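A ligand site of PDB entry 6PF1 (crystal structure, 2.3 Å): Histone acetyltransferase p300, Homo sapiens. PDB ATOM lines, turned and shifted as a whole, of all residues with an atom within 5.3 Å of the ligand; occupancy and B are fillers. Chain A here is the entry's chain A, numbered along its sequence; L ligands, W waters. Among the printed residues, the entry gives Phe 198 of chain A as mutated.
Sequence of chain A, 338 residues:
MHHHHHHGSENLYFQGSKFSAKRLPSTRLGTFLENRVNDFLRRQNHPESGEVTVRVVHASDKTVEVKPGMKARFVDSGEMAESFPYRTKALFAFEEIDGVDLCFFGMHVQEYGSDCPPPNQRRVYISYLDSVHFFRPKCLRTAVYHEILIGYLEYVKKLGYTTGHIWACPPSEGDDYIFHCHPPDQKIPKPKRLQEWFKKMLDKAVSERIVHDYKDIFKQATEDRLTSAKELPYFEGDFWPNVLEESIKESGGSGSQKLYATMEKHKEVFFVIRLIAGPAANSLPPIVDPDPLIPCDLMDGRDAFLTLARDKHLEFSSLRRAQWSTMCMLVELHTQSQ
The backbone nitrogen of Pro 189 sits close to a nitrogen (N4) of the ligand (3.4 Å). Asp 130 touches the ligand. Tyr 145 touches the ligand. Trp 167 touches the ligand (O to C21, 3.6 Å). Cys 169 touches the ligand (O to C20, 3.6 Å). CA of Pro 170 touches O16 of the ligand (3.9 Å). Pro 171 touches the ligand (CD to O16, 3.6 Å). Tyr 177 touches the ligand (CE2 to N7, 3.7 Å). NE2 of Gln 186 touches O15 of the ligand, at 3.8 Å. CB of Lys 187 touches N4 of the ligand, 3.5 Å away. Leu 194 touches the ligand. Of the 27 residues printed, 18 come within 4 Å of the ligand. The nearest printed residue that does not touch the ligand is Tyr 128 (4.04 Å).
Water W9 lies within hydrogen-bond range of O14 of the ligand, NE2 of Gln 186 and O of Lys 187. Water W3 bridges an oxygen (O12) of the ligand and the guanidinium group of Arg 141. Water W2 bridges an oxygen (O9) of the ligand (2.7 Å) and the guanidinium group of Arg 193 (3.3 Å). Water W10 lies within hydrogen-bond range of O5 of the ligand (2.8 Å), NH1 of Arg 141 (3.0 Å) and O of Lys 138 (3.5 Å). Water W1 bridges S1 of the ligand (3.1 Å) and O of Ser 127 (3.5 Å). Water W4 bridges the side-chain amino group (NZ) of Lys 138 and an oxygen (O5) of the ligand.
N of Tyr 177 lies within hydrogen-bond range of OD2 of Asp 130, 3.4 Å away. O of Ser 131 sits at hydrogen-bond distance from NE2 of His 182, at 3.2 Å. The backbone carbonyl oxygen (O) of Ser 131 sits at hydrogen-bond distance from the side-chain amide nitrogen (NE2) of Gln 186. The side-chain hydroxyl of Ser 131 lies within hydrogen-bond range of the side-chain hydroxyl of Tyr 145 (3.3 Å). The side-chain carboxylate of Asp 130 is in hydrogen-bond range of a ring nitrogen (NE2) of His 182 (2.8 Å). O of Cys 169 sits at hydrogen-bond distance from OH of Tyr 177, at 2.7 Å. NH1 of Arg 141 lies within hydrogen-bond range of O of Lys 138, 3.2 Å away. The side-chain hydroxyl (OH) of Tyr 177 lies close to the backbone carbonyl oxygen (O) of Pro 170 (3.4 Å).
An oxygen (O15) of the ligand lies within hydrogen-bond range of the side-chain hydroxyl of Ser 131 (2.9 Å). NE of Arg 141 lies within salt-bridge range of O12 of the ligand. N7 of the ligand sits at hydrogen-bond distance from O of Leu 129, 3.2 Å away. O of Ile 188 is in hydrogen-bond range of N3 of the ligand (3.0 Å). The guanidinium group (NH1) of Arg 193 is in hydrogen-bond range of an oxygen (O6) of the ligand, 3.0 Å away. The backbone NH (N) of Leu 129 lies close to a sulfur (S1) of the ligand (3.7 Å). O15 of the ligand sits at hydrogen-bond distance from N of Ser 131, 3.2 Å away. The indole nitrogen of Trp 197 is in hydrogen-bond range of an oxygen (O11) of the ligand (2.7 Å). OG1 of Thr 142 is in hydrogen-bond range of O11 of the ligand, 2.7 Å away.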
ATOM      1  N   PHE A 105     -19.932  27.021 -32.475  1.00  0.00           N
ATOM      2  CA  PHE A 105     -20.405  26.582 -31.187  1.00  0.00           C
ATOM      3  C   PHE A 105     -19.252  26.189 -30.256  1.00  0.00           C
ATOM      4  O   PHE A 105     -18.243  25.678 -30.714  1.00  0.00           O
ATOM      5  CB  PHE A 105     -21.383  25.436 -31.421  1.00  0.00           C
ATOM      6  CG  PHE A 105     -21.805  24.718 -30.198  1.00  0.00           C
ATOM      7  CD1 PHE A 105     -21.009  23.683 -29.660  1.00  0.00           C
ATOM      8  CD2 PHE A 105     -23.014  25.038 -29.571  1.00  0.00           C
ATOM      9  CE1 PHE A 105     -21.406  22.983 -28.519  1.00  0.00           C
ATOM     10  CE2 PHE A 105     -23.409  24.344 -28.417  1.00  0.00           C
ATOM     11  CZ  PHE A 105     -22.601  23.331 -27.898  1.00  0.00           C
ATOM     12  N   ILE A 126     -22.018  20.758 -17.379  1.00  0.00           N
ATOM     13  CA  ILE A 126     -21.735  21.703 -18.463  1.00  0.00           C
ATOM     14  C   ILE A 126     -21.525  23.088 -17.872  1.00  0.00           C
ATOM     15  O   ILE A 126     -22.501  23.711 -17.526  1.00  0.00           O
ATOM     16  CB  ILE A 126     -22.860  21.694 -19.500  1.00  0.00           C
ATOM     17  CG1 ILE A 126     -22.948  20.309 -20.098  1.00  0.00           C
ATOM     18  CG2 ILE A 126     -22.599  22.713 -20.592  1.00  0.00           C
ATOM     19  CD1 ILE A 126     -23.925  20.177 -21.239  1.00  0.00           C
ATOM     20  N   SER A 127     -20.271  23.539 -17.750  1.00  0.00           N
ATOM     21  CA  SER A 127     -20.014  24.837 -17.109  1.00  0.00           C
ATOM     22  C   SER A 127     -20.611  26.014 -17.928  1.00  0.00           C
ATOM     23  O   SER A 127     -21.160  26.968 -17.352  1.00  0.00           O
ATOM     24  CB  SER A 127     -18.512  25.144 -16.889  1.00  0.00           C
ATOM     25  OG  SER A 127     -17.657  24.022 -16.962  1.00  0.00           O
ATOM     26  N   TYR A 128     -20.438  25.926 -19.245  1.00  0.00           N
ATOM     27  CA  TYR A 128     -20.606  27.046 -20.163  1.00  0.00           C
ATOM     28  C   TYR A 128     -20.784  26.469 -21.553  1.00  0.00           C
ATOM     29  O   TYR A 128     -20.064  25.566 -21.947  1.00  0.00           O
ATOM     30  CB  TYR A 128     -19.331  27.931 -20.231  1.00  0.00           C
ATOM     31  CG  TYR A 128     -19.150  28.829 -19.024  1.00  0.00           C
ATOM     32  CD1 TYR A 128     -19.951  29.952 -18.864  1.00  0.00           C
ATOM     33  CD2 TYR A 128     -18.204  28.526 -18.038  1.00  0.00           C
ATOM     34  CE1 TYR A 128     -19.827  30.771 -17.754  1.00  0.00           C
ATOM     35  CE2 TYR A 128     -18.073  29.336 -16.909  1.00  0.00           C
ATOM     36  CZ  TYR A 128     -18.887  30.463 -16.765  1.00  0.00           C
ATOM     37  OH  TYR A 128     -18.762  31.304 -15.665  1.00  0.00           O
ATOM     38  N   LEU A 129     -21.720  27.057 -22.288  1.00  0.00           N
ATOM     39  CA  LEU A 129     -22.041  26.688 -23.654  1.00  0.00           C
ATOM     40  C   LEU A 129     -22.395  28.001 -24.387  1.00  0.00           C
ATOM     41  O   LEU A 129     -22.958  28.919 -23.793  1.00  0.00           O
ATOM     42  CB  LEU A 129     -23.235  25.735 -23.573  1.00  0.00           C
ATOM     43  CG  LEU A 129     -24.109  25.212 -24.709  1.00  0.00           C
ATOM     44  CD1 LEU A 129     -25.204  24.389 -24.048  1.00  0.00           C
ATOM     45  CD2 LEU A 129     -24.775  26.246 -25.601  1.00  0.00           C
ATOM     46  N   ASP A 130     -22.049  28.124 -25.652  1.00  0.00           N
ATOM     47  CA  ASP A 130     -22.308  29.380 -26.356  1.00  0.00           C
ATOM     48  C   ASP A 130     -22.266  29.072 -27.851  1.00  0.00           C
ATOM     49  O   ASP A 130     -21.715  28.027 -28.275  1.00  0.00           O
ATOM     50  CB  ASP A 130     -21.232  30.425 -25.985  1.00  0.00           C
ATOM     51  CG  ASP A 130     -21.644  31.895 -26.265  1.00  0.00           C
ATOM     52  OD1 ASP A 130     -22.757  32.176 -26.740  1.00  0.00           O
ATOM     53  OD2 ASP A 130     -20.813  32.790 -25.982  1.00  0.00           O
ATOM     54  N   SER A 131     -22.874  29.960 -28.620  1.00  0.00           N
ATOM     55  CA  SER A 131     -22.893  29.831 -30.035  1.00  0.00           C
ATOM     56  C   SER A 131     -23.047  31.147 -30.748  1.00  0.00           C
ATOM     57  O   SER A 131     -23.424  32.181 -30.169  1.00  0.00           O
ATOM     58  CB  SER A 131     -24.079  28.989 -30.462  1.00  0.00           C
ATOM     59  OG  SER A 131     -25.226  29.788 -30.389  1.00  0.00           O
ATOM     60  N   LYS A 138     -29.812  27.648 -41.779  1.00  0.00           N
ATOM     61  CA  LYS A 138     -30.271  28.121 -40.487  1.00  0.00           C
ATOM     62  C   LYS A 138     -31.371  27.262 -39.920  1.00  0.00           C
ATOM     63  O   LYS A 138     -31.575  27.263 -38.723  1.00  0.00           O
ATOM     64  CB  LYS A 138     -30.712  29.595 -40.601  1.00  0.00           C
ATOM     65  CG  LYS A 138     -31.761  29.825 -41.697  1.00  0.00           C
ATOM     66  CD  LYS A 138     -31.987  31.293 -41.961  1.00  0.00           C
ATOM     67  CE  LYS A 138     -32.672  31.967 -40.788  1.00  0.00           C
ATOM     68  NZ  LYS A 138     -33.473  33.076 -41.361  1.00  0.00           N
ATOM     69  N   ARG A 141     -29.872  24.598 -37.595  1.00  0.00           N
ATOM     70  CA  ARG A 141     -29.026  25.122 -36.527  1.00  0.00           C
ATOM     71  C   ARG A 141     -29.330  24.472 -35.154  1.00  0.00           C
ATOM     72  O   ARG A 141     -28.473  23.838 -34.544  1.00  0.00           O
ATOM     73  CB  ARG A 141     -29.157  26.666 -36.438  1.00  0.00           C
ATOM     74  CG  ARG A 141     -28.263  27.247 -35.348  1.00  0.00           C
ATOM     75  CD  ARG A 141     -28.376  28.741 -35.112  1.00  0.00           C
ATOM     76  NE  ARG A 141     -29.697  29.108 -34.634  1.00  0.00           N
ATOM     77  CZ  ARG A 141     -30.720  29.508 -35.396  1.00  0.00           C
ATOM     78  NH1 ARG A 141     -30.597  29.590 -36.707  1.00  0.00           N
ATOM     79  NH2 ARG A 141     -31.881  29.827 -34.821  1.00  0.00           N
ATOM     80  N   THR A 142     -30.537  24.695 -34.662  1.00  0.00           N
ATOM     81  CA  THR A 142     -30.970  24.120 -33.418  1.00  0.00           C
ATOM     82  C   THR A 142     -30.763  22.593 -33.383  1.00  0.00           C
ATOM     83  O   THR A 142     -30.225  22.048 -32.420  1.00  0.00           O
ATOM     84  CB  THR A 142     -32.421  24.544 -33.122  1.00  0.00           C
ATOM     85  OG1 THR A 142     -32.458  25.961 -32.923  1.00  0.00           O
ATOM     86  CG2 THR A 142     -32.955  23.852 -31.881  1.00  0.00           C
ATOM     87  N   TYR A 145     -27.010  21.791 -32.747  1.00  0.00           N
ATOM     88  CA  TYR A 145     -26.659  22.025 -31.337  1.00  0.00           C
ATOM     89  C   TYR A 145     -27.153  20.859 -30.485  1.00  0.00           C
ATOM     90  O   TYR A 145     -26.451  20.371 -29.593  1.00  0.00           O
ATOM     91  CB  TYR A 145     -27.257  23.302 -30.796  1.00  0.00           C
ATOM     92  CG  TYR A 145     -26.865  24.580 -31.468  1.00  0.00           C
ATOM     93  CD1 TYR A 145     -25.655  24.712 -32.134  1.00  0.00           C
ATOM     94  CD2 TYR A 145     -27.661  25.720 -31.348  1.00  0.00           C
ATOM     95  CE1 TYR A 145     -25.284  25.919 -32.683  1.00  0.00           C
ATOM     96  CE2 TYR A 145     -27.303  26.938 -31.924  1.00  0.00           C
ATOM     97  CZ  TYR A 145     -26.111  27.023 -32.597  1.00  0.00           C
ATOM     98  OH  TYR A 145     -25.714  28.180 -33.190  1.00  0.00           O
ATOM     99  N   TRP A 167     -27.124  23.731 -16.011  1.00  0.00           N
ATOM    100  CA  TRP A 167     -27.643  24.978 -15.474  1.00  0.00           C
ATOM    101  C   TRP A 167     -28.072  25.810 -16.711  1.00  0.00           C
ATOM    102  O   TRP A 167     -27.248  26.117 -17.566  1.00  0.00           O
ATOM    103  CB  TRP A 167     -26.526  25.654 -14.653  1.00  0.00           C
ATOM    104  CG  TRP A 167     -26.858  26.965 -14.037  1.00  0.00           C
ATOM    105  CD1 TRP A 167     -28.078  27.515 -13.947  1.00  0.00           C
ATOM    106  CD2 TRP A 167     -25.946  27.900 -13.381  1.00  0.00           C
ATOM    107  NE1 TRP A 167     -28.022  28.721 -13.301  1.00  0.00           N
ATOM    108  CE2 TRP A 167     -26.723  28.999 -12.946  1.00  0.00           C
ATOM    109  CE3 TRP A 167     -24.563  27.904 -13.130  1.00  0.00           C
ATOM    110  CZ2 TRP A 167     -26.170  30.110 -12.279  1.00  0.00           C
ATOM    111  CZ3 TRP A 167     -24.003  29.022 -12.467  1.00  0.00           C
ATOM    112  CH2 TRP A 167     -24.813  30.098 -12.048  1.00  0.00           C
ATOM    113  N   ALA A 168     -29.360  26.139 -16.801  1.00  0.00           N
ATOM    114  CA  ALA A 168     -29.902  26.944 -17.885  1.00  0.00           C
ATOM    115  C   ALA A 168     -30.064  28.401 -17.461  1.00  0.00           C
ATOM    116  O   ALA A 168     -31.150  28.871 -17.194  1.00  0.00           O
ATOM    117  CB  ALA A 168     -31.230  26.371 -18.334  1.00  0.00           C
ATOM    118  N   CYS A 169     -28.954  29.108 -17.385  1.00  0.00           N
ATOM    119  CA  CYS A 169     -28.935  30.529 -17.140  1.00  0.00           C
ATOM    120  C   CYS A 169     -28.483  31.256 -18.426  1.00  0.00           C
ATOM    121  O   CYS A 169     -27.339  31.140 -18.834  1.00  0.00           O
ATOM    122  CB  CYS A 169     -27.949  30.811 -16.008  1.00  0.00           C
ATOM    123  SG  CYS A 169     -28.087  32.453 -15.257  1.00  0.00           S
ATOM    124  N   PRO A 170     -29.374  32.024 -19.063  1.00  0.00           N
ATOM    125  CA  PRO A 170     -28.839  32.841 -20.166  1.00  0.00           C
ATOM    126  C   PRO A 170     -27.935  33.950 -19.631  1.00  0.00           C
ATOM    127  O   PRO A 170     -28.100  34.352 -18.501  1.00  0.00           O
ATOM    128  CB  PRO A 170     -30.090  33.440 -20.851  1.00  0.00           C
ATOM    129  CG  PRO A 170     -31.173  33.324 -19.855  1.00  0.00           C
ATOM    130  CD  PRO A 170     -30.808  32.273 -18.837  1.00  0.00           C
ATOM    131  N   PRO A 171     -26.960  34.428 -20.436  1.00  0.00           N
ATOM    132  CA  PRO A 171     -26.126  35.570 -20.033  1.00  0.00           C
ATOM    133  C   PRO A 171     -26.934  36.862 -19.825  1.00  0.00           C
ATOM    134  O   PRO A 171     -27.844  37.128 -20.586  1.00  0.00           O
ATOM    135  CB  PRO A 171     -25.196  35.764 -21.241  1.00  0.00           C
ATOM    136  CG  PRO A 171     -25.994  35.246 -22.374  1.00  0.00           C
ATOM    137  CD  PRO A 171     -26.721  34.038 -21.833  1.00  0.00           C
ATOM    138  N   TYR A 177     -20.461  34.570 -23.079  1.00  0.00           N
ATOM    139  CA  TYR A 177     -20.018  33.409 -22.327  1.00  0.00           C
ATOM    140  C   TYR A 177     -18.719  32.885 -22.854  1.00  0.00           C
ATOM    141  O   TYR A 177     -17.823  32.592 -22.086  1.00  0.00           O
ATOM    142  CB  TYR A 177     -21.082  32.311 -22.312  1.00  0.00           C
ATOM    143  CG  TYR A 177     -22.169  32.433 -21.246  1.00  0.00           C
ATOM    144  CD1 TYR A 177     -22.074  33.322 -20.166  1.00  0.00           C
ATOM    145  CD2 TYR A 177     -23.275  31.639 -21.314  1.00  0.00           C
ATOM    146  CE1 TYR A 177     -23.050  33.395 -19.185  1.00  0.00           C
ATOM    147  CE2 TYR A 177     -24.277  31.709 -20.353  1.00  0.00           C
ATOM    148  CZ  TYR A 177     -24.168  32.585 -19.298  1.00  0.00           C
ATOM    149  OH  TYR A 177     -25.160  32.640 -18.347  1.00  0.00           O
ATOM    150  N   HIS A 182     -21.245  39.071 -29.853  1.00  0.00           N
ATOM    151  CA  HIS A 182     -22.265  38.402 -30.634  1.00  0.00           C
ATOM    152  C   HIS A 182     -22.871  39.331 -31.658  1.00  0.00           C
ATOM    153  O   HIS A 182     -22.770  40.531 -31.533  1.00  0.00           O
ATOM    154  CB  HIS A 182     -23.375  37.853 -29.731  1.00  0.00           C
ATOM    155  CG  HIS A 182     -22.970  36.627 -28.998  1.00  0.00           C
ATOM    156  ND1 HIS A 182     -21.940  36.607 -28.084  1.00  0.00           N
ATOM    157  CD2 HIS A 182     -23.403  35.357 -29.087  1.00  0.00           C
ATOM    158  CE1 HIS A 182     -21.777  35.388 -27.622  1.00  0.00           C
ATOM    159  NE2 HIS A 182     -22.672  34.610 -28.211  1.00  0.00           N
ATOM    160  N   GLN A 186     -28.603  38.559 -32.946  1.00  0.00           N
ATOM    161  CA  GLN A 186     -28.764  37.253 -32.259  1.00  0.00           C
ATOM    162  C   GLN A 186     -29.460  37.467 -30.949  1.00  0.00           C
ATOM    163  O   GLN A 186     -28.851  37.927 -29.985  1.00  0.00           O
ATOM    164  CB  GLN A 186     -27.445  36.490 -32.049  1.00  0.00           C
ATOM    165  CG  GLN A 186     -27.607  35.101 -31.403  1.00  0.00           C
ATOM    166  CD  GLN A 186     -26.321  34.260 -31.427  1.00  0.00           C
ATOM    167  OE1 GLN A 186     -25.495  34.406 -32.325  1.00  0.00           O
ATOM    168  NE2 GLN A 186     -26.178  33.346 -30.452  1.00  0.00           N
ATOM    169  N   LYS A 187     -30.739  37.091 -30.907  1.00  0.00           N
ATOM    170  CA  LYS A 187     -31.561  37.250 -29.712  1.00  0.00           C
ATOM    171  C   LYS A 187     -31.029  36.312 -28.642  1.00  0.00           C
ATOM    172  O   LYS A 187     -30.545  35.216 -28.955  1.00  0.00           O
ATOM    173  CB  LYS A 187     -33.032  36.960 -30.007  1.00  0.00           C
ATOM    174  CG  LYS A 187     -33.641  37.918 -31.036  1.00  0.00           C
ATOM    175  CD  LYS A 187     -35.157  37.953 -30.951  1.00  0.00           C
ATOM    176  CE  LYS A 187     -35.772  38.897 -31.965  1.00  0.00           C
ATOM    177  NZ  LYS A 187     -35.458  38.499 -33.360  1.00  0.00           N
ATOM    178  N   ILE A 188     -31.102  36.772 -27.394  1.00  0.00           N
ATOM    179  CA  ILE A 188     -30.754  35.990 -26.224  1.00  0.00           C
ATOM    180  C   ILE A 188     -32.054  35.441 -25.674  1.00  0.00           C
ATOM    181  O   ILE A 188     -32.990  36.196 -25.443  1.00  0.00           O
ATOM    182  CB  ILE A 188     -30.029  36.841 -25.144  1.00  0.00           C
ATOM    183  CG1 ILE A 188     -28.707  37.422 -25.681  1.00  0.00           C
ATOM    184  CG2 ILE A 188     -29.830  36.087 -23.835  1.00  0.00           C
ATOM    185  CD1 ILE A 188     -27.793  36.419 -26.368  1.00  0.00           C
ATOM    186  N   PRO A 189     -32.142  34.128 -25.466  1.00  0.00           N
ATOM    187  CA  PRO A 189     -33.419  33.617 -24.967  1.00  0.00           C
ATOM    188  C   PRO A 189     -33.623  34.003 -23.495  1.00  0.00           C
ATOM    189  O   PRO A 189     -32.665  34.148 -22.767  1.00  0.00           O
ATOM    190  CB  PRO A 189     -33.293  32.104 -25.164  1.00  0.00           C
ATOM    191  CG  PRO A 189     -31.830  31.832 -25.156  1.00  0.00           C
ATOM    192  CD  PRO A 189     -31.199  33.038 -25.801  1.00  0.00           C
ATOM    193  N   LYS A 190     -34.884  34.192 -23.122  1.00  0.00           N
ATOM    194  CA  LYS A 190     -35.261  34.384 -21.724  1.00  0.00           C
ATOM    195  C   LYS A 190     -35.201  32.998 -21.076  1.00  0.00           C
ATOM    196  O   LYS A 190     -35.242  31.957 -21.771  1.00  0.00           O
ATOM    197  CB  LYS A 190     -36.668  35.017 -21.611  1.00  0.00           C
ATOM    198  N   ARG A 193     -37.668  30.169 -22.406  1.00  0.00           N
ATOM    199  CA  ARG A 193     -37.328  29.633 -23.716  1.00  0.00           C
ATOM    200  C   ARG A 193     -36.090  28.704 -23.638  1.00  0.00           C
ATOM    201  O   ARG A 193     -36.064  27.675 -24.308  1.00  0.00           O
ATOM    202  CB  ARG A 193     -37.116  30.771 -24.708  1.00  0.00           C
ATOM    203  CG  ARG A 193     -36.572  30.364 -26.057  1.00  0.00           C
ATOM    204  CD  ARG A 193     -36.270  31.581 -26.901  1.00  0.00           C
ATOM    205  NE  ARG A 193     -37.483  32.243 -27.344  1.00  0.00           N
ATOM    206  CZ  ARG A 193     -38.264  31.818 -28.318  1.00  0.00           C
ATOM    207  NH1 ARG A 193     -38.015  30.691 -28.978  1.00  0.00           N
ATOM    208  NH2 ARG A 193     -39.341  32.518 -28.632  1.00  0.00           N
ATOM    209  N   LEU A 194     -35.098  29.030 -22.802  1.00  0.00           N
ATOM    210  CA  LEU A 194     -33.886  28.184 -22.650  1.00  0.00           C
ATOM    211  C   LEU A 194     -34.154  26.886 -21.914  1.00  0.00           C
ATOM    212  O   LEU A 194     -33.547  25.873 -22.195  1.00  0.00           O
ATOM    213  CB  LEU A 194     -32.768  28.938 -21.921  1.00  0.00           C
ATOM    214  CG  LEU A 194     -31.374  28.280 -21.793  1.00  0.00           C
ATOM    215  CD1 LEU A 194     -30.717  28.003 -23.148  1.00  0.00           C
ATOM    216  CD2 LEU A 194     -30.439  29.124 -20.926  1.00  0.00           C
ATOM    217  N   TRP A 197     -35.791  24.697 -24.436  1.00  0.00           N
ATOM    218  CA  TRP A 197     -34.760  24.260 -25.394  1.00  0.00           C
ATOM    219  C   TRP A 197     -33.988  23.021 -24.860  1.00  0.00           C
ATOM    220  O   TRP A 197     -33.717  22.067 -25.572  1.00  0.00           O
ATOM    221  CB  TRP A 197     -33.805  25.447 -25.656  1.00  0.00           C
ATOM    222  CG  TRP A 197     -32.840  25.308 -26.769  1.00  0.00           C
ATOM    223  CD1 TRP A 197     -33.014  25.693 -28.058  1.00  0.00           C
ATOM    224  CD2 TRP A 197     -31.502  24.809 -26.685  1.00  0.00           C
ATOM    225  NE1 TRP A 197     -31.881  25.441 -28.794  1.00  0.00           N
ATOM    226  CE2 TRP A 197     -30.940  24.895 -27.977  1.00  0.00           C
ATOM    227  CE3 TRP A 197     -30.735  24.282 -25.657  1.00  0.00           C
ATOM    228  CZ2 TRP A 197     -29.631  24.501 -28.268  1.00  0.00           C
ATOM    229  CZ3 TRP A 197     -29.425  23.886 -25.924  1.00  0.00           C
ATOM    230  CH2 TRP A 197     -28.892  23.984 -27.242  1.00  0.00           C
ATOM    231  N   PHE A 198     -33.621  23.071 -23.586  1.00  0.00           N
ATOM    232  CA  PHE A 198     -32.946  21.935 -22.954  1.00  0.00           C
ATOM    233  C   PHE A 198     -33.873  20.718 -22.800  1.00  0.00           C
ATOM    234  O   PHE A 198     -33.392  19.579 -22.935  1.00  0.00           O
ATOM    235  CB  PHE A 198     -32.384  22.319 -21.587  1.00  0.00           C
ATOM    236  CG  PHE A 198     -31.082  23.030 -21.656  1.00  0.00           C
ATOM    237  CD1 PHE A 198     -29.967  22.404 -22.167  1.00  0.00           C
ATOM    238  CD2 PHE A 198     -30.945  24.347 -21.173  1.00  0.00           C
ATOM    239  CE1 PHE A 198     -28.752  23.053 -22.227  1.00  0.00           C
ATOM    240  CE2 PHE A 198     -29.737  24.981 -21.217  1.00  0.00           C
ATOM    241  CZ  PHE A 198     -28.643  24.345 -21.753  1.00  0.00           C
HETATM  242  N1  LIG L   1     -37.438  36.744 -27.993  1.00  0.00           N
HETATM  243  C1  LIG L   1     -37.957  36.281 -29.147  1.00  0.00           C
HETATM  244  N2  LIG L   1     -37.362  35.311 -29.855  1.00  0.00           N
HETATM  245  C2  LIG L   1     -36.203  34.741 -29.416  1.00  0.00           C
HETATM  246  C3  LIG L   1     -35.572  35.198 -28.171  1.00  0.00           C
HETATM  247  C4  LIG L   1     -36.282  36.289 -27.466  1.00  0.00           C
HETATM  248  N3  LIG L   1     -35.750  36.774 -26.331  1.00  0.00           N
HETATM  249  N4  LIG L   1     -34.452  34.495 -27.971  1.00  0.00           N
HETATM  250  C5  LIG L   1     -34.371  33.647 -29.032  1.00  0.00           C
HETATM  251  N5  LIG L   1     -35.417  33.786 -29.873  1.00  0.00           N
HETATM  252  C6  LIG L   1     -35.682  33.066 -31.137  1.00  0.00           C
HETATM  253  C7  LIG L   1     -34.502  33.173 -32.070  1.00  0.00           C
HETATM  254  O1  LIG L   1     -34.466  34.434 -32.727  1.00  0.00           O
HETATM  255  C8  LIG L   1     -34.736  32.000 -32.969  1.00  0.00           C
HETATM  256  O2  LIG L   1     -35.675  32.248 -34.009  1.00  0.00           O
HETATM  257  P1  LIG L   1     -35.453  31.473 -35.381  1.00  0.00           P
HETATM  258  O3  LIG L   1     -35.420  30.007 -35.038  1.00  0.00           O
HETATM  259  O4  LIG L   1     -36.624  31.913 -36.237  1.00  0.00           O
HETATM  260  O5  LIG L   1     -34.170  32.057 -35.898  1.00  0.00           O
HETATM  261  C9  LIG L   1     -35.360  30.963 -32.026  1.00  0.00           C
HETATM  262  O6  LIG L   1     -35.908  31.678 -30.946  1.00  0.00           O
HETATM  263  C10 LIG L   1     -34.311  29.962 -31.560  1.00  0.00           C
HETATM  264  O7  LIG L   1     -33.213  30.616 -30.884  1.00  0.00           O
HETATM  265  P2  LIG L   1     -32.554  30.081 -29.509  1.00  0.00           P
HETATM  266  O8  LIG L   1     -31.433  31.039 -29.190  1.00  0.00           O
HETATM  267  O9  LIG L   1     -33.541  29.825 -28.421  1.00  0.00           O
HETATM  268  O10 LIG L   1     -32.091  28.586 -29.978  1.00  0.00           O
HETATM  269  P3  LIG L   1     -30.734  28.240 -30.769  1.00  0.00           P
HETATM  270  O11 LIG L   1     -30.844  26.754 -30.964  1.00  0.00           O
HETATM  271  O12 LIG L   1     -30.551  29.138 -31.936  1.00  0.00           O
HETATM  272  O13 LIG L   1     -29.572  28.701 -29.736  1.00  0.00           O
HETATM  273  C11 LIG L   1     -28.304  28.787 -27.708  1.00  0.00           C
HETATM  274  C12 LIG L   1     -29.635  28.420 -28.339  1.00  0.00           C
HETATM  275  C13 LIG L   1     -28.369  28.419 -26.208  1.00  0.00           C
HETATM  276  C14 LIG L   1     -27.180  27.987 -28.375  1.00  0.00           C
HETATM  277  C15 LIG L   1     -28.102  30.284 -27.978  1.00  0.00           C
HETATM  278  O14 LIG L   1     -29.263  31.077 -27.712  1.00  0.00           O
HETATM  279  C16 LIG L   1     -26.969  30.870 -27.212  1.00  0.00           C
HETATM  280  O15 LIG L   1     -25.876  30.724 -27.701  1.00  0.00           O
HETATM  281  N6  LIG L   1     -27.199  31.529 -26.076  1.00  0.00           N
HETATM  282  C17 LIG L   1     -26.106  32.020 -25.228  1.00  0.00           C
HETATM  283  C18 LIG L   1     -25.421  30.897 -24.407  1.00  0.00           C
HETATM  284  C19 LIG L   1     -26.320  30.290 -23.347  1.00  0.00           C
HETATM  285  O16 LIG L   1     -27.395  30.813 -23.225  1.00  0.00           O
HETATM  286  N7  LIG L   1     -25.897  29.252 -22.570  1.00  0.00           N
HETATM  287  C20 LIG L   1     -26.674  28.803 -21.427  1.00  0.00           C
HETATM  288  C21 LIG L   1     -26.309  27.497 -20.714  1.00  0.00           C
HETATM  289  S1  LIG L   1     -24.616  27.484 -20.054  1.00  0.00           S
HETATM  290  O   HOH W   1     -24.216  28.577 -17.206  1.00  0.00           O
HETATM  291  O   HOH W   2     -35.761  28.350 -28.804  1.00  0.00           O
HETATM  292  O   HOH W   3     -29.125  31.297 -32.179  1.00  0.00           O
HETATM  293  O   HOH W   4     -34.863  33.046 -38.731  1.00  0.00           O
HETATM  294  O   HOH W   5     -32.729  28.554 -25.904  1.00  0.00           O
HETATM  295  O   HOH W   6     -30.734  33.089 -30.773  1.00  0.00           O
HETATM  296  O   HOH W   7     -38.907  34.858 -31.707  1.00  0.00           O
HETATM  297  O   HOH W   8     -37.298  34.433 -25.146  1.00  0.00           O
HETATM  298  O   HOH W   9     -28.262  33.237 -28.702  1.00  0.00           O
HETATM  299  O   HOH W  10     -33.362  30.137 -37.832  1.00  0.00           O
